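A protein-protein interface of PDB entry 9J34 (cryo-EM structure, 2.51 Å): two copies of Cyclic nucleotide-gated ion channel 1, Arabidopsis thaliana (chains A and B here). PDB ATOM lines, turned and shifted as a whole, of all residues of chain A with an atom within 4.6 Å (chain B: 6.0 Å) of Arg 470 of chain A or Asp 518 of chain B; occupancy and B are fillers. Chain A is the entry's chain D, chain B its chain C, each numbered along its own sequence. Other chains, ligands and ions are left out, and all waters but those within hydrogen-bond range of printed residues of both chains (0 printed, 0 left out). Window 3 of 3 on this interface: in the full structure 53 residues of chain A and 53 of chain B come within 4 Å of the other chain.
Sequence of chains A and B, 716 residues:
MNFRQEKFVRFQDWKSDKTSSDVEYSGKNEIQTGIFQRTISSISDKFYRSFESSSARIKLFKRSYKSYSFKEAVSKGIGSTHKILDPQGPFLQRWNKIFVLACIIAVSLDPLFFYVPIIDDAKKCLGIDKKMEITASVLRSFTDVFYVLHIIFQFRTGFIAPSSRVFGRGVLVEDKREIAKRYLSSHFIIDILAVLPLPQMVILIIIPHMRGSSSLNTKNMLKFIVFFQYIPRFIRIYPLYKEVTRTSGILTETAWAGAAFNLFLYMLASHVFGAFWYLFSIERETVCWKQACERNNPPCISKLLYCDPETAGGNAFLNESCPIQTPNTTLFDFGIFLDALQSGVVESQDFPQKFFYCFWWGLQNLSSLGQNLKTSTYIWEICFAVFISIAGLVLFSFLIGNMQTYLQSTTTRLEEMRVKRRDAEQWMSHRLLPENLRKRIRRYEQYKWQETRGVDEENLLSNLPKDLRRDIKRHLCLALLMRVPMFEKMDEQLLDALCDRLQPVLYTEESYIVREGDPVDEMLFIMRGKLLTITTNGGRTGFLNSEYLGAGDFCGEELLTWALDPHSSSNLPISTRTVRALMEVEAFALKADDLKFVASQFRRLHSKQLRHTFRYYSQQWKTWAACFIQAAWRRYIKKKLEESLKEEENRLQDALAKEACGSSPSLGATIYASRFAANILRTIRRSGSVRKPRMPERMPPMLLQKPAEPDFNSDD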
ATOM      1  N   LYS A 466       0.481  -0.738   8.531  1.00  0.00           N
ATOM      2  CA  LYS A 466       1.618  -0.707   7.620  1.00  0.00           C
ATOM      3  C   LYS A 466       1.708   0.577   6.805  1.00  0.00           C
ATOM      4  O   LYS A 466       2.793   0.899   6.317  1.00  0.00           O
ATOM      5  CB  LYS A 466       1.600  -1.918   6.679  1.00  0.00           C
ATOM      6  CG  LYS A 466       0.905  -1.686   5.340  1.00  0.00           C
ATOM      7  CD  LYS A 466       1.171  -2.784   4.320  1.00  0.00           C
ATOM      8  CE  LYS A 466       2.623  -3.246   4.339  1.00  0.00           C
ATOM      9  NZ  LYS A 466       2.923  -4.187   3.229  1.00  0.00           N
ATOM     10  N   ASP A 467       0.615   1.325   6.651  1.00  0.00           N
ATOM     11  CA  ASP A 467       0.704   2.600   5.954  1.00  0.00           C
ATOM     12  C   ASP A 467       0.981   3.743   6.911  1.00  0.00           C
ATOM     13  O   ASP A 467       1.574   4.752   6.513  1.00  0.00           O
ATOM     14  CB  ASP A 467      -0.574   2.879   5.155  1.00  0.00           C
ATOM     15  CG  ASP A 467      -1.746   3.284   6.036  1.00  0.00           C
ATOM     16  OD1 ASP A 467      -2.207   2.457   6.847  1.00  0.00           O
ATOM     17  OD2 ASP A 467      -2.218   4.436   5.901  1.00  0.00           O
ATOM     18  N   LEU A 468       0.576   3.596   8.170  1.00  0.00           N
ATOM     19  CA  LEU A 468       0.875   4.606   9.174  1.00  0.00           C
ATOM     20  C   LEU A 468       2.330   4.506   9.611  1.00  0.00           C
ATOM     21  O   LEU A 468       2.997   5.524   9.816  1.00  0.00           O
ATOM     22  CB  LEU A 468      -0.090   4.439  10.345  1.00  0.00           C
ATOM     23  CG  LEU A 468      -0.270   5.476  11.445  1.00  0.00           C
ATOM     24  CD1 LEU A 468      -1.713   5.436  11.888  1.00  0.00           C
ATOM     25  CD2 LEU A 468       0.603   5.138  12.607  1.00  0.00           C
ATOM     26  N   ARG A 469       2.839   3.277   9.736  1.00  0.00           N
ATOM     27  CA  ARG A 469       4.259   3.055   9.991  1.00  0.00           C
ATOM     28  C   ARG A 469       5.119   3.500   8.814  1.00  0.00           C
ATOM     29  O   ARG A 469       6.270   3.908   9.001  1.00  0.00           O
ATOM     30  CB  ARG A 469       4.493   1.576  10.301  1.00  0.00           C
ATOM     31  CG  ARG A 469       5.895   1.209  10.750  1.00  0.00           C
ATOM     32  CD  ARG A 469       6.155  -0.262  10.532  1.00  0.00           C
ATOM     33  NE  ARG A 469       5.003  -1.067  10.919  1.00  0.00           N
ATOM     34  CZ  ARG A 469       4.475  -2.022  10.165  1.00  0.00           C
ATOM     35  NH1 ARG A 469       4.994  -2.293   8.976  1.00  0.00           N
ATOM     36  NH2 ARG A 469       3.426  -2.705  10.598  1.00  0.00           N
ATOM     37  N   ARG A 470       4.576   3.437   7.597  1.00  0.00           N
ATOM     38  CA  ARG A 470       5.308   3.902   6.426  1.00  0.00           C
ATOM     39  C   ARG A 470       5.400   5.422   6.395  1.00  0.00           C
ATOM     40  O   ARG A 470       6.437   5.979   6.019  1.00  0.00           O
ATOM     41  CB  ARG A 470       4.635   3.380   5.159  1.00  0.00           C
ATOM     42  CG  ARG A 470       5.386   3.682   3.888  1.00  0.00           C
ATOM     43  CD  ARG A 470       4.442   3.839   2.711  1.00  0.00           C
ATOM     44  NE  ARG A 470       3.848   2.570   2.302  1.00  0.00           N
ATOM     45  CZ  ARG A 470       2.541   2.337   2.244  1.00  0.00           C
ATOM     46  NH1 ARG A 470       1.677   3.286   2.573  1.00  0.00           N
ATOM     47  NH2 ARG A 470       2.100   1.150   1.856  1.00  0.00           N
ATOM     48  N   ASP A 471       4.328   6.111   6.798  1.00  0.00           N
ATOM     49  CA  ASP A 471       4.329   7.569   6.777  1.00  0.00           C
ATOM     50  C   ASP A 471       5.219   8.154   7.863  1.00  0.00           C
ATOM     51  O   ASP A 471       5.725   9.270   7.706  1.00  0.00           O
ATOM     52  CB  ASP A 471       2.904   8.102   6.915  1.00  0.00           C
ATOM     53  CG  ASP A 471       2.130   8.046   5.612  1.00  0.00           C
ATOM     54  OD1 ASP A 471       1.298   8.947   5.374  1.00  0.00           O
ATOM     55  OD2 ASP A 471       2.350   7.102   4.826  1.00  0.00           O
ATOM     56  N   ILE A 472       5.409   7.436   8.970  1.00  0.00           N
ATOM     57  CA  ILE A 472       6.315   7.907  10.013  1.00  0.00           C
ATOM     58  C   ILE A 472       7.762   7.763   9.563  1.00  0.00           C
ATOM     59  O   ILE A 472       8.561   8.700   9.669  1.00  0.00           O
ATOM     60  CB  ILE A 472       6.065   7.148  11.325  1.00  0.00           C
ATOM     61  CG1 ILE A 472       4.684   7.471  11.884  1.00  0.00           C
ATOM     62  CG2 ILE A 472       7.126   7.491  12.347  1.00  0.00           C
ATOM     63  CD1 ILE A 472       4.163   6.397  12.784  1.00  0.00           C
ATOM     64  N   LYS A 473       8.113   6.589   9.040  1.00  0.00           N
ATOM     65  CA  LYS A 473       9.489   6.321   8.649  1.00  0.00           C
ATOM     66  C   LYS A 473       9.895   7.066   7.386  1.00  0.00           C
ATOM     67  O   LYS A 473      11.092   7.249   7.152  1.00  0.00           O
ATOM     68  CB  LYS A 473       9.691   4.817   8.477  1.00  0.00           C
ATOM     69  CG  LYS A 473       9.855   4.085   9.795  1.00  0.00           C
ATOM     70  CD  LYS A 473       9.707   2.588   9.631  1.00  0.00           C
ATOM     71  CE  LYS A 473      10.522   1.845  10.674  1.00  0.00           C
ATOM     72  NZ  LYS A 473      10.305   0.375  10.614  1.00  0.00           N
ATOM     73  N   ARG A 474       8.939   7.498   6.565  1.00  0.00           N
ATOM     74  CA  ARG A 474       9.266   8.398   5.469  1.00  0.00           C
ATOM     75  C   ARG A 474       9.458   9.829   5.940  1.00  0.00           C
ATOM     76  O   ARG A 474      10.065  10.630   5.224  1.00  0.00           O
ATOM     77  CB  ARG A 474       8.179   8.357   4.397  1.00  0.00           C
ATOM     78  CG  ARG A 474       8.236   7.131   3.516  1.00  0.00           C
ATOM     79  CD  ARG A 474       7.179   7.193   2.430  1.00  0.00           C
ATOM     80  NE  ARG A 474       7.667   7.881   1.240  1.00  0.00           N
ATOM     81  CZ  ARG A 474       7.318   9.113   0.885  1.00  0.00           C
ATOM     82  NH1 ARG A 474       6.465   9.811   1.625  1.00  0.00           N
ATOM     83  NH2 ARG A 474       7.823   9.647  -0.217  1.00  0.00           N
ATOM     84  N   GLN A 493       9.272   2.355  -4.106  1.00  0.00           N
ATOM     85  CA  GLN A 493       9.024   0.980  -3.695  1.00  0.00           C
ATOM     86  C   GLN A 493      10.230   0.303  -3.074  1.00  0.00           C
ATOM     87  O   GLN A 493      10.063  -0.731  -2.419  1.00  0.00           O
ATOM     88  CB  GLN A 493       8.556   0.128  -4.891  1.00  0.00           C
ATOM     89  CG  GLN A 493       7.257   0.582  -5.560  1.00  0.00           C
ATOM     90  CD  GLN A 493       6.052   0.682  -4.631  1.00  0.00           C
ATOM     91  OE1 GLN A 493       5.970   0.009  -3.602  1.00  0.00           O
ATOM     92  NE2 GLN A 493       5.095   1.526  -5.011  1.00  0.00           N
ATOM     93  N   ASP A 496      11.228   2.631   0.241  1.00  0.00           N
ATOM     94  CA  ASP A 496      10.288   2.267   1.292  1.00  0.00           C
ATOM     95  C   ASP A 496      10.656   0.948   1.941  1.00  0.00           C
ATOM     96  O   ASP A 496      10.239   0.685   3.071  1.00  0.00           O
ATOM     97  CB  ASP A 496       8.871   2.213   0.749  1.00  0.00           C
ATOM     98  CG  ASP A 496       8.232   3.566   0.726  1.00  0.00           C
ATOM     99  OD1 ASP A 496       7.366   3.816  -0.131  1.00  0.00           O
ATOM    100  OD2 ASP A 496       8.621   4.406   1.544  1.00  0.00           O
ATOM    101  N   TYR B 512      -5.131   3.643   4.659  1.00  0.00           N
ATOM    102  CA  TYR B 512      -4.893   2.980   3.389  1.00  0.00           C
ATOM    103  C   TYR B 512      -4.534   1.522   3.629  1.00  0.00           C
ATOM    104  O   TYR B 512      -3.584   1.220   4.356  1.00  0.00           O
ATOM    105  CB  TYR B 512      -3.768   3.672   2.623  1.00  0.00           C
ATOM    106  CG  TYR B 512      -4.189   4.920   1.889  1.00  0.00           C
ATOM    107  CD1 TYR B 512      -4.536   4.872   0.547  1.00  0.00           C
ATOM    108  CD2 TYR B 512      -4.231   6.149   2.538  1.00  0.00           C
ATOM    109  CE1 TYR B 512      -4.917   6.011  -0.130  1.00  0.00           C
ATOM    110  CE2 TYR B 512      -4.612   7.296   1.869  1.00  0.00           C
ATOM    111  CZ  TYR B 512      -4.953   7.219   0.536  1.00  0.00           C
ATOM    112  OH  TYR B 512      -5.332   8.358  -0.132  1.00  0.00           O
ATOM    113  N   ILE B 513      -5.297   0.622   3.017  1.00  0.00           N
ATOM    114  CA  ILE B 513      -4.965  -0.796   3.067  1.00  0.00           C
ATOM    115  C   ILE B 513      -3.800  -1.098   2.144  1.00  0.00           C
ATOM    116  O   ILE B 513      -2.789  -1.687   2.542  1.00  0.00           O
ATOM    117  CB  ILE B 513      -6.187  -1.644   2.684  1.00  0.00           C
ATOM    118  CG1 ILE B 513      -7.437  -1.151   3.412  1.00  0.00           C
ATOM    119  CG2 ILE B 513      -5.885  -3.096   2.904  1.00  0.00           C
ATOM    120  CD1 ILE B 513      -7.395  -1.329   4.887  1.00  0.00           C
ATOM    121  N   VAL B 514      -3.943  -0.702   0.882  1.00  0.00           N
ATOM    122  CA  VAL B 514      -2.911  -0.859  -0.130  1.00  0.00           C
ATOM    123  C   VAL B 514      -3.087   0.298  -1.101  1.00  0.00           C
ATOM    124  O   VAL B 514      -4.155   0.909  -1.184  1.00  0.00           O
ATOM    125  CB  VAL B 514      -3.003  -2.242  -0.831  1.00  0.00           C
ATOM    126  CG1 VAL B 514      -4.138  -2.283  -1.845  1.00  0.00           C
ATOM    127  CG2 VAL B 514      -1.673  -2.642  -1.463  1.00  0.00           C
ATOM    128  N   ARG B 515      -2.009   0.648  -1.786  1.00  0.00           N
ATOM    129  CA  ARG B 515      -2.035   1.641  -2.842  1.00  0.00           C
ATOM    130  C   ARG B 515      -1.643   0.968  -4.147  1.00  0.00           C
ATOM    131  O   ARG B 515      -1.038  -0.108  -4.154  1.00  0.00           O
ATOM    132  CB  ARG B 515      -1.088   2.801  -2.542  1.00  0.00           C
ATOM    133  CG  ARG B 515      -1.241   3.358  -1.147  1.00  0.00           C
ATOM    134  CD  ARG B 515      -0.065   4.241  -0.794  1.00  0.00           C
ATOM    135  NE  ARG B 515      -0.224   4.882   0.506  1.00  0.00           N
ATOM    136  CZ  ARG B 515      -0.791   6.068   0.693  1.00  0.00           C
ATOM    137  NH1 ARG B 515      -1.261   6.751  -0.343  1.00  0.00           N
ATOM    138  NH2 ARG B 515      -0.890   6.571   1.914  1.00  0.00           N
ATOM    139  N   GLU B 516      -2.005   1.607  -5.254  1.00  0.00           N
ATOM    140  CA  GLU B 516      -1.677   1.059  -6.560  1.00  0.00           C
ATOM    141  C   GLU B 516      -0.182   1.184  -6.813  1.00  0.00           C
ATOM    142  O   GLU B 516       0.378   2.283  -6.771  1.00  0.00           O
ATOM    143  CB  GLU B 516      -2.474   1.778  -7.646  1.00  0.00           C
ATOM    144  CG  GLU B 516      -2.368   1.151  -9.020  1.00  0.00           C
ATOM    145  CD  GLU B 516      -3.453   1.643  -9.949  1.00  0.00           C
ATOM    146  OE1 GLU B 516      -4.574   1.895  -9.462  1.00  0.00           O
ATOM    147  OE2 GLU B 516      -3.186   1.790 -11.159  1.00  0.00           O
ATOM    148  N   GLY B 517       0.462   0.052  -7.075  1.00  0.00           N
ATOM    149  CA  GLY B 517       1.897  -0.005  -7.219  1.00  0.00           C
ATOM    150  C   GLY B 517       2.620  -0.776  -6.135  1.00  0.00           C
ATOM    151  O   GLY B 517       3.738  -1.247  -6.377  1.00  0.00           O
ATOM    152  N   ASP B 518       2.012  -0.925  -4.942  1.00  0.00           N
ATOM    153  CA  ASP B 518       2.629  -1.647  -3.844  1.00  0.00           C
ATOM    154  C   ASP B 518       2.480  -3.152  -4.045  1.00  0.00           C
ATOM    155  O   ASP B 518       1.515  -3.610  -4.669  1.00  0.00           O
ATOM    156  CB  ASP B 518       1.982  -1.260  -2.509  1.00  0.00           C
ATOM    157  CG  ASP B 518       2.346   0.141  -2.060  1.00  0.00           C
ATOM    158  OD1 ASP B 518       3.549   0.478  -2.087  1.00  0.00           O
ATOM    159  OD2 ASP B 518       1.442   0.893  -1.655  1.00  0.00           O
ATOM    160  N   PRO B 519       3.419  -3.957  -3.549  1.00  0.00           N
ATOM    161  CA  PRO B 519       3.200  -5.407  -3.541  1.00  0.00           C
ATOM    162  C   PRO B 519       2.165  -5.784  -2.495  1.00  0.00           C
ATOM    163  O   PRO B 519       2.087  -5.181  -1.421  1.00  0.00           O
ATOM    164  CB  PRO B 519       4.580  -5.976  -3.201  1.00  0.00           C
ATOM    165  CG  PRO B 519       5.259  -4.882  -2.460  1.00  0.00           C
ATOM    166  CD  PRO B 519       4.774  -3.604  -3.090  1.00  0.00           C
ATOM    167  N   VAL B 520       1.356  -6.786  -2.828  1.00  0.00           N
ATOM    168  CA  VAL B 520       0.241  -7.206  -1.987  1.00  0.00           C
ATOM    169  C   VAL B 520       0.726  -8.292  -1.032  1.00  0.00           C
ATOM    170  O   VAL B 520       1.026  -9.413  -1.450  1.00  0.00           O
ATOM    171  CB  VAL B 520      -0.942  -7.696  -2.830  1.00  0.00           C
ATOM    172  CG1 VAL B 520      -2.080  -8.114  -1.938  1.00  0.00           C
ATOM    173  CG2 VAL B 520      -1.399  -6.614  -3.772  1.00  0.00           C
ATOM    174  N   GLU B 558      -5.849 -10.604  -5.824  1.00  0.00           N
ATOM    175  CA  GLU B 558      -4.753 -10.737  -6.770  1.00  0.00           C
ATOM    176  C   GLU B 558      -3.776 -11.806  -6.319  1.00  0.00           C
ATOM    177  O   GLU B 558      -3.057 -12.373  -7.148  1.00  0.00           O
ATOM    178  CB  GLU B 558      -3.961  -9.427  -6.912  1.00  0.00           C
ATOM    179  CG  GLU B 558      -4.679  -8.217  -7.560  1.00  0.00           C
ATOM    180  CD  GLU B 558      -3.894  -6.913  -7.624  1.00  0.00           C
ATOM    181  OE1 GLU B 558      -2.817  -6.818  -7.001  1.00  0.00           O
ATOM    182  OE2 GLU B 558      -4.361  -5.980  -8.305  1.00  0.00           O
ATOM    183  N   PRO B 573       2.561 -10.011  -6.274  1.00  0.00           N
ATOM    184  CA  PRO B 573       1.895  -9.281  -7.357  1.00  0.00           C
ATOM    185  C   PRO B 573       1.638  -7.832  -6.986  1.00  0.00           C
ATOM    186  O   PRO B 573       1.380  -7.490  -5.829  1.00  0.00           O
ATOM    187  CB  PRO B 573       0.580 -10.049  -7.551  1.00  0.00           C
ATOM    188  CG  PRO B 573       0.378 -10.801  -6.282  1.00  0.00           C
ATOM    189  CD  PRO B 573       1.748 -11.145  -5.803  1.00  0.00           C
ATOM    190  N   ILE B 574       1.724  -6.978  -7.994  1.00  0.00           N
ATOM    191  CA  ILE B 574       1.600  -5.537  -7.824  1.00  0.00           C
ATOM    192  C   ILE B 574       0.119  -5.194  -7.760  1.00  0.00           C
ATOM    193  O   ILE B 574      -0.674  -5.687  -8.572  1.00  0.00           O
ATOM    194  CB  ILE B 574       2.308  -4.797  -8.971  1.00  0.00           C
ATOM    195  CG1 ILE B 574       3.806  -5.111  -8.954  1.00  0.00           C
ATOM    196  CG2 ILE B 574       2.106  -3.301  -8.878  1.00  0.00           C
ATOM    197  CD1 ILE B 574       4.492  -4.756  -7.651  1.00  0.00           C
ATOM    198  N   SER B 575      -0.258  -4.383  -6.773  1.00  0.00           N
ATOM    199  CA  SER B 575      -1.654  -4.023  -6.573  1.00  0.00           C
ATOM    200  C   SER B 575      -2.171  -3.164  -7.718  1.00  0.00           C
ATOM    201  O   SER B 575      -1.556  -2.165  -8.099  1.00  0.00           O
ATOM    202  CB  SER B 575      -1.833  -3.266  -5.260  1.00  0.00           C
ATOM    203  OG  SER B 575      -3.196  -2.942  -5.054  1.00  0.00           O
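The backbone NH of Tyr 512 of chain B lies within hydrogen-bond range of the side-chain carboxylate of Asp 467 of chain A, at 3.3 Å.
The guanidinium group (NH2) of Arg 470 of chain A lies within salt-bridge range of the side-chain carboxylate (OD2) of Asp 518 of chain B.
NE2 of Gln 493 of chain A is in hydrogen-bond range of O of Gly 517 of chain B.
The side-chain amide oxygen (OE1) of Gln 493 of chain A sits close to the side-chain carboxylate (OD1) of Asp 518 of chain B, 2.9 Å away.
The guanidinium group of Arg 470 of chain A lies close to the guanidinium group of Arg 515 of chain B (3.2 Å).
The side-chain carboxylate (OD2) of Asp 518 of chain B lies close to the backbone NH (N) of Arg 515 of chain B.
The backbone NH (N) of Gly 517 of chain B sits at hydrogen-bond distance from the backbone carbonyl oxygen (O) of Ser 575 of chain B, 3.2 Å away.
The backbone NH (N) of Ser 575 of chain B sits at hydrogen-bond distance from the backbone carbonyl oxygen (O) of Asp 518 of chain B (2.9 Å).
Among the printed residues, pairs that only touch across the chains: Gln 493 of chain A with Pro 519 of chain B (3.8 Å).
Of the printed residues of chain B, Asp 467 of chain A touches Tyr 512 (3.1 Å).
Printed residues of chain B within 4 Å of Arg 470 of chain A: Arg 515 (3.2 Å) and Asp 518 (3.6 Å).
Val 514 of chain B touches none of the printed residues of chain A.
Of the printed residues of chain A, Gly 517 of chain B touches Gln 493 (3.4 Å).
Asp 518 of chain B touches two residues of chain A.
Printed residues of chain A within 4 Å of Pro 519 of chain B: Gln 493.
Glu 558 of chain B touches none of the printed residues of chain A.
The nearest residue of chain B that does not touch Arg 470 of chain A is Tyr 512 of chain B (5.5 Å).
The nearest printed residue of chain A that does not touch Asp 518 of chain B is Asp 496 of chain A (5.4 Å).
The nearest printed residue of chain A that does not touch Pro 519 of chain B is Lys 466 of chain A (4.8 Å).
Of the 13 printed residues of chain B, 5 touch a printed residue of chain A.
Hydrophobic or aromatic side chains of chain B within 4 Å of the printed part of chain A: Tyr 512 and Pro 519.
Printed residues of chain A that touch a printed residue of chain B: Asp 467, Arg 470 and Gln 493.
Along chain A the printed residues that touch a printed residue of chain B span positions 467 to 493.
Among the printed residues, 6 pairs touch across the chains.
Among the printed residues, Asp or Glu carboxylates within 4 Å of a Lys or Arg side-chain nitrogen of the other chain: Arg 470 of chain A with Asp 518 of chain B.
No position is printed for both chains.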
